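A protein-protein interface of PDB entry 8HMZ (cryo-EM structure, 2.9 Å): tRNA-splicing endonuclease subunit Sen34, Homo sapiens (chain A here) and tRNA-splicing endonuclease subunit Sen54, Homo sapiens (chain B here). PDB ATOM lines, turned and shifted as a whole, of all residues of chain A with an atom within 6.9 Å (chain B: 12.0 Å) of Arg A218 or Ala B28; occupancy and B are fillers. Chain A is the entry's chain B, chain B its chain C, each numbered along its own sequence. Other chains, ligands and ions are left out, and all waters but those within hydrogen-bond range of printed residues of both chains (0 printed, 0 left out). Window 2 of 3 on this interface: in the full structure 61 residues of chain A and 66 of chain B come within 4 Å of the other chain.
The side-chain amide nitrogen (NE2) of Gln B162 lies within hydrogen-bond range of the backbone carbonyl oxygen (O) of Pro A92 (3.1 Å).
O of Val B30 is in hydrogen-bond range of N of Ala A217 (3.0 Å).
The guanidinium group of Arg A218 lies within hydrogen-bond range of the backbone carbonyl oxygen of Ala B28 (2.7 Å).
The backbone carbonyl oxygen (O) of Arg A218 lies within hydrogen-bond range of the side-chain hydroxyl (OG) of Ser A90 (3.0 Å).
Among the printed residues, pairs that only touch across the chains: Lys A216 with Glu B31 (3.3 Å), Val A89 with Val B30 (3.5 Å), Lys A216 with Val B30 (3.6 Å), Ala A217 with Ala B29 (3.6 Å) and Pro A219 with Ala B28 (3.9 Å).
Of chain B, only Val B30 comes within 4 Å of Val A89.
No residue of chain B comes within 4 Å of Ser A90.
Of the printed residues of chain B, Lys A216 touches Val B30 (3.6 Å) and Glu B31 (3.3 Å).
Of chain B, only Ala B29 (3.6 Å) and Val B30 (3.0 Å) come within 4 Å of Ala A217.
Arg A218 touches just one residue of chain B: Ala B28 (2.7 Å).
No residue of chain B comes within 4 Å of Leu A220.
Of chain A, only Arg A218 and Pro A219 come within 4 Å of Ala B28.
Printed residues of chain A within 4 Å of Ala B29: Ala A217 (3.6 Å).
Of the printed residues of chain A, Val B30 touches Val A89 (3.5 Å), Lys A216 (3.6 Å) and Ala A217 (3.0 Å).
Gln B158 touches none of the printed residues of chain A.
The nearest residue of chain A that does not touch Ala B28 is Ala A217 (5.1 Å).
Hydrophobic or aromatic side chains of chain A within 4 Å of the printed part of chain B: Val A89 and Pro A219.
Of the 8 printed residues of chain B, 5 touch a printed residue of chain A.
Hydrophobic or aromatic side chains of chain B that line the printed part of chain A: Ala B29 and Val B30.
Among the printed residues, no Asp or Glu carboxylate lies within 4 Å of a Lys or Arg side-chain nitrogen of the other chain.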
ATOM      1  N   LEU A  88      24.363 -18.479  -6.925  1.00  0.00           N
ATOM      2  CA  LEU A  88      24.728 -19.810  -6.458  1.00  0.00           C
ATOM      3  C   LEU A  88      24.358 -19.952  -4.990  1.00  0.00           C
ATOM      4  O   LEU A  88      24.936 -19.288  -4.125  1.00  0.00           O
ATOM      5  CB  LEU A  88      26.216 -20.072  -6.673  1.00  0.00           C
ATOM      6  CG  LEU A  88      26.783 -19.768  -8.058  1.00  0.00           C
ATOM      7  CD1 LEU A  88      28.290 -19.670  -7.995  1.00  0.00           C
ATOM      8  CD2 LEU A  88      26.365 -20.833  -9.050  1.00  0.00           C
ATOM      9  N   VAL A  89      23.377 -20.798  -4.709  1.00  0.00           N
ATOM     10  CA  VAL A  89      23.030 -21.149  -3.353  1.00  0.00           C
ATOM     11  C   VAL A  89      23.555 -22.552  -3.061  1.00  0.00           C
ATOM     12  O   VAL A  89      23.975 -23.280  -3.954  1.00  0.00           O
ATOM     13  CB  VAL A  89      21.509 -21.058  -3.103  1.00  0.00           C
ATOM     14  CG1 VAL A  89      21.006 -19.681  -3.446  1.00  0.00           C
ATOM     15  CG2 VAL A  89      20.771 -22.111  -3.908  1.00  0.00           C
ATOM     16  N   SER A  90      23.535 -22.929  -1.791  1.00  0.00           N
ATOM     17  CA  SER A  90      23.804 -24.298  -1.382  1.00  0.00           C
ATOM     18  C   SER A  90      22.478 -25.023  -1.211  1.00  0.00           C
ATOM     19  O   SER A  90      21.508 -24.449  -0.708  1.00  0.00           O
ATOM     20  CB  SER A  90      24.609 -24.329  -0.083  1.00  0.00           C
ATOM     21  OG  SER A  90      24.296 -23.221   0.736  1.00  0.00           O
ATOM     22  N   ALA A  91      22.438 -26.278  -1.648  1.00  0.00           N
ATOM     23  CA  ALA A  91      21.189 -27.024  -1.679  1.00  0.00           C
ATOM     24  C   ALA A  91      20.578 -27.084  -0.282  1.00  0.00           C
ATOM     25  O   ALA A  91      21.235 -27.556   0.655  1.00  0.00           O
ATOM     26  CB  ALA A  91      21.422 -28.436  -2.212  1.00  0.00           C
ATOM     27  N   PRO A  92      19.343 -26.622  -0.099  1.00  0.00           N
ATOM     28  CA  PRO A  92      18.775 -26.551   1.251  1.00  0.00           C
ATOM     29  C   PRO A  92      18.562 -27.930   1.849  1.00  0.00           C
ATOM     30  O   PRO A  92      18.697 -28.967   1.197  1.00  0.00           O
ATOM     31  CB  PRO A  92      17.439 -25.823   1.051  1.00  0.00           C
ATOM     32  CG  PRO A  92      17.479 -25.265  -0.325  1.00  0.00           C
ATOM     33  CD  PRO A  92      18.415 -26.110  -1.118  1.00  0.00           C
ATOM     34  N   LYS A 216      14.144 -21.555   1.795  1.00  0.00           N
ATOM     35  CA  LYS A 216      15.167 -20.529   1.918  1.00  0.00           C
ATOM     36  C   LYS A 216      16.528 -21.201   1.917  1.00  0.00           C
ATOM     37  O   LYS A 216      16.771 -22.124   2.699  1.00  0.00           O
ATOM     38  CB  LYS A 216      14.996 -19.700   3.193  1.00  0.00           C
ATOM     39  CG  LYS A 216      13.568 -19.537   3.655  1.00  0.00           C
ATOM     40  CD  LYS A 216      13.488 -18.568   4.820  1.00  0.00           C
ATOM     41  CE  LYS A 216      13.463 -17.126   4.344  1.00  0.00           C
ATOM     42  NZ  LYS A 216      12.414 -16.898   3.313  1.00  0.00           N
ATOM     43  N   ALA A 217      17.406 -20.738   1.040  1.00  0.00           N
ATOM     44  CA  ALA A 217      18.765 -21.233   0.957  1.00  0.00           C
ATOM     45  C   ALA A 217      19.723 -20.111   1.325  1.00  0.00           C
ATOM     46  O   ALA A 217      19.338 -18.942   1.413  1.00  0.00           O
ATOM     47  CB  ALA A 217      19.081 -21.772  -0.441  1.00  0.00           C
ATOM     48  N   ARG A 218      20.977 -20.477   1.549  1.00  0.00           N
ATOM     49  CA  ARG A 218      21.973 -19.488   1.906  1.00  0.00           C
ATOM     50  C   ARG A 218      22.966 -19.335   0.769  1.00  0.00           C
ATOM     51  O   ARG A 218      23.450 -20.343   0.237  1.00  0.00           O
ATOM     52  CB  ARG A 218      22.699 -19.886   3.197  1.00  0.00           C
ATOM     53  CG  ARG A 218      23.355 -18.712   3.904  1.00  0.00           C
ATOM     54  CD  ARG A 218      22.697 -18.425   5.244  1.00  0.00           C
ATOM     55  NE  ARG A 218      23.148 -17.152   5.798  1.00  0.00           N
ATOM     56  CZ  ARG A 218      23.317 -16.915   7.095  1.00  0.00           C
ATOM     57  NH1 ARG A 218      23.068 -17.868   7.984  1.00  0.00           N
ATOM     58  NH2 ARG A 218      23.733 -15.724   7.504  1.00  0.00           N
ATOM     59  N   PRO A 219      23.280 -18.106   0.364  1.00  0.00           N
ATOM     60  CA  PRO A 219      24.118 -17.910  -0.823  1.00  0.00           C
ATOM     61  C   PRO A 219      25.515 -18.479  -0.637  1.00  0.00           C
ATOM     62  O   PRO A 219      26.110 -18.390   0.438  1.00  0.00           O
ATOM     63  CB  PRO A 219      24.146 -16.387  -0.983  1.00  0.00           C
ATOM     64  CG  PRO A 219      23.829 -15.868   0.378  1.00  0.00           C
ATOM     65  CD  PRO A 219      22.816 -16.824   0.913  1.00  0.00           C
ATOM     66  N   LEU A 220      26.032 -19.067  -1.709  1.00  0.00           N
ATOM     67  CA  LEU A 220      27.358 -19.659  -1.727  1.00  0.00           C
ATOM     68  C   LEU A 220      28.392 -18.627  -2.152  1.00  0.00           C
ATOM     69  O   LEU A 220      28.117 -17.737  -2.960  1.00  0.00           O
ATOM     70  CB  LEU A 220      27.390 -20.856  -2.678  1.00  0.00           C
ATOM     71  CG  LEU A 220      28.656 -21.706  -2.716  1.00  0.00           C
ATOM     72  CD1 LEU A 220      28.599 -22.764  -1.644  1.00  0.00           C
ATOM     73  CD2 LEU A 220      28.838 -22.338  -4.082  1.00  0.00           C
ATOM     74  N   ASP A 221      29.595 -18.760  -1.601  1.00  0.00           N
ATOM     75  CA  ASP A 221      30.715 -17.879  -1.912  1.00  0.00           C
ATOM     76  C   ASP A 221      31.683 -18.649  -2.803  1.00  0.00           C
ATOM     77  O   ASP A 221      32.309 -19.615  -2.357  1.00  0.00           O
ATOM     78  CB  ASP A 221      31.405 -17.401  -0.638  1.00  0.00           C
ATOM     79  CG  ASP A 221      32.328 -16.236  -0.886  1.00  0.00           C
ATOM     80  OD1 ASP A 221      32.393 -15.781  -2.042  1.00  0.00           O
ATOM     81  OD2 ASP A 221      32.989 -15.775   0.067  1.00  0.00           O
ATOM     82  N   ASP A 228      31.056 -27.280  -0.497  1.00  0.00           N
ATOM     83  CA  ASP A 228      30.258 -27.397  -1.715  1.00  0.00           C
ATOM     84  C   ASP A 228      30.734 -26.433  -2.790  1.00  0.00           C
ATOM     85  O   ASP A 228      29.959 -25.998  -3.644  1.00  0.00           O
ATOM     86  CB  ASP A 228      28.786 -27.172  -1.396  1.00  0.00           C
ATOM     87  CG  ASP A 228      28.571 -25.992  -0.484  1.00  0.00           C
ATOM     88  OD1 ASP A 228      29.573 -25.374  -0.067  1.00  0.00           O
ATOM     89  OD2 ASP A 228      27.406 -25.685  -0.175  1.00  0.00           O
ATOM     90  N   ALA B  28      22.878 -13.070   4.718  1.00  0.00           N
ATOM     91  CA  ALA B  28      21.445 -13.036   4.450  1.00  0.00           C
ATOM     92  C   ALA B  28      20.925 -14.425   4.093  1.00  0.00           C
ATOM     93  O   ALA B  28      21.590 -15.428   4.351  1.00  0.00           O
ATOM     94  CB  ALA B  28      21.138 -12.051   3.335  1.00  0.00           C
ATOM     95  N   ALA B  29      19.736 -14.479   3.495  1.00  0.00           N
ATOM     96  CA  ALA B  29      19.142 -15.751   3.091  1.00  0.00           C
ATOM     97  C   ALA B  29      18.177 -15.492   1.947  1.00  0.00           C
ATOM     98  O   ALA B  29      17.148 -14.839   2.143  1.00  0.00           O
ATOM     99  CB  ALA B  29      18.424 -16.421   4.261  1.00  0.00           C
ATOM    100  N   VAL B  30      18.508 -15.997   0.766  1.00  0.00           N
ATOM    101  CA  VAL B  30      17.664 -15.833  -0.411  1.00  0.00           C
ATOM    102  C   VAL B  30      16.582 -16.904  -0.412  1.00  0.00           C
ATOM    103  O   VAL B  30      16.833 -18.065  -0.073  1.00  0.00           O
ATOM    104  CB  VAL B  30      18.520 -15.882  -1.689  1.00  0.00           C
ATOM    105  CG1 VAL B  30      19.435 -17.084  -1.663  1.00  0.00           C
ATOM    106  CG2 VAL B  30      17.642 -15.906  -2.931  1.00  0.00           C
ATOM    107  N   GLU B  31      15.372 -16.517  -0.802  1.00  0.00           N
ATOM    108  CA  GLU B  31      14.215 -17.404  -0.804  1.00  0.00           C
ATOM    109  C   GLU B  31      14.025 -17.940  -2.217  1.00  0.00           C
ATOM    110  O   GLU B  31      13.613 -17.202  -3.118  1.00  0.00           O
ATOM    111  CB  GLU B  31      12.969 -16.671  -0.313  1.00  0.00           C
ATOM    112  CG  GLU B  31      11.834 -17.584   0.115  1.00  0.00           C
ATOM    113  CD  GLU B  31      10.754 -17.716  -0.938  1.00  0.00           C
ATOM    114  OE1 GLU B  31      11.065 -17.603  -2.140  1.00  0.00           O
ATOM    115  OE2 GLU B  31       9.587 -17.934  -0.558  1.00  0.00           O
ATOM    116  N   VAL B  32      14.333 -19.219  -2.403  1.00  0.00           N
ATOM    117  CA  VAL B  32      14.257 -19.889  -3.699  1.00  0.00           C
ATOM    118  C   VAL B  32      12.798 -20.129  -4.073  1.00  0.00           C
ATOM    119  O   VAL B  32      12.075 -20.801  -3.324  1.00  0.00           O
ATOM    120  CB  VAL B  32      15.040 -21.211  -3.676  1.00  0.00           C
ATOM    121  CG1 VAL B  32      14.843 -21.975  -4.967  1.00  0.00           C
ATOM    122  CG2 VAL B  32      16.511 -20.951  -3.430  1.00  0.00           C
ATOM    123  N   PRO B  33      12.319 -19.613  -5.200  1.00  0.00           N
ATOM    124  CA  PRO B  33      10.980 -19.975  -5.670  1.00  0.00           C
ATOM    125  C   PRO B  33      10.993 -21.399  -6.208  1.00  0.00           C
ATOM    126  O   PRO B  33      12.043 -21.962  -6.516  1.00  0.00           O
ATOM    127  CB  PRO B  33      10.713 -18.955  -6.776  1.00  0.00           C
ATOM    128  CG  PRO B  33      12.064 -18.684  -7.339  1.00  0.00           C
ATOM    129  CD  PRO B  33      13.037 -18.779  -6.181  1.00  0.00           C
ATOM    130  N   GLN B 158      13.957 -33.490  -7.782  1.00  0.00           N
ATOM    131  CA  GLN B 158      15.023 -32.683  -7.198  1.00  0.00           C
ATOM    132  C   GLN B 158      15.359 -33.155  -5.788  1.00  0.00           C
ATOM    133  O   GLN B 158      16.532 -33.371  -5.451  1.00  0.00           O
ATOM    134  CB  GLN B 158      14.613 -31.213  -7.182  1.00  0.00           C
ATOM    135  CG  GLN B 158      15.661 -30.293  -6.605  1.00  0.00           C
ATOM    136  CD  GLN B 158      15.328 -28.839  -6.808  1.00  0.00           C
ATOM    137  OE1 GLN B 158      16.094 -27.959  -6.424  1.00  0.00           O
ATOM    138  NE2 GLN B 158      14.174 -28.574  -7.397  1.00  0.00           N
ATOM    139  N   GLN B 162      18.741 -35.022  -4.361  1.00  0.00           N
ATOM    140  CA  GLN B 162      19.534 -34.494  -3.257  1.00  0.00           C
ATOM    141  C   GLN B 162      19.667 -35.489  -2.109  1.00  0.00           C
ATOM    142  O   GLN B 162      20.731 -35.570  -1.485  1.00  0.00           O
ATOM    143  CB  GLN B 162      18.922 -33.184  -2.759  1.00  0.00           C
ATOM    144  CG  GLN B 162      19.154 -32.889  -1.291  1.00  0.00           C
ATOM    145  CD  GLN B 162      18.311 -31.737  -0.793  1.00  0.00           C
ATOM    146  OE1 GLN B 162      18.054 -30.781  -1.522  1.00  0.00           O
ATOM    147  NE2 GLN B 162      17.877 -31.820   0.458  1.00  0.00           N
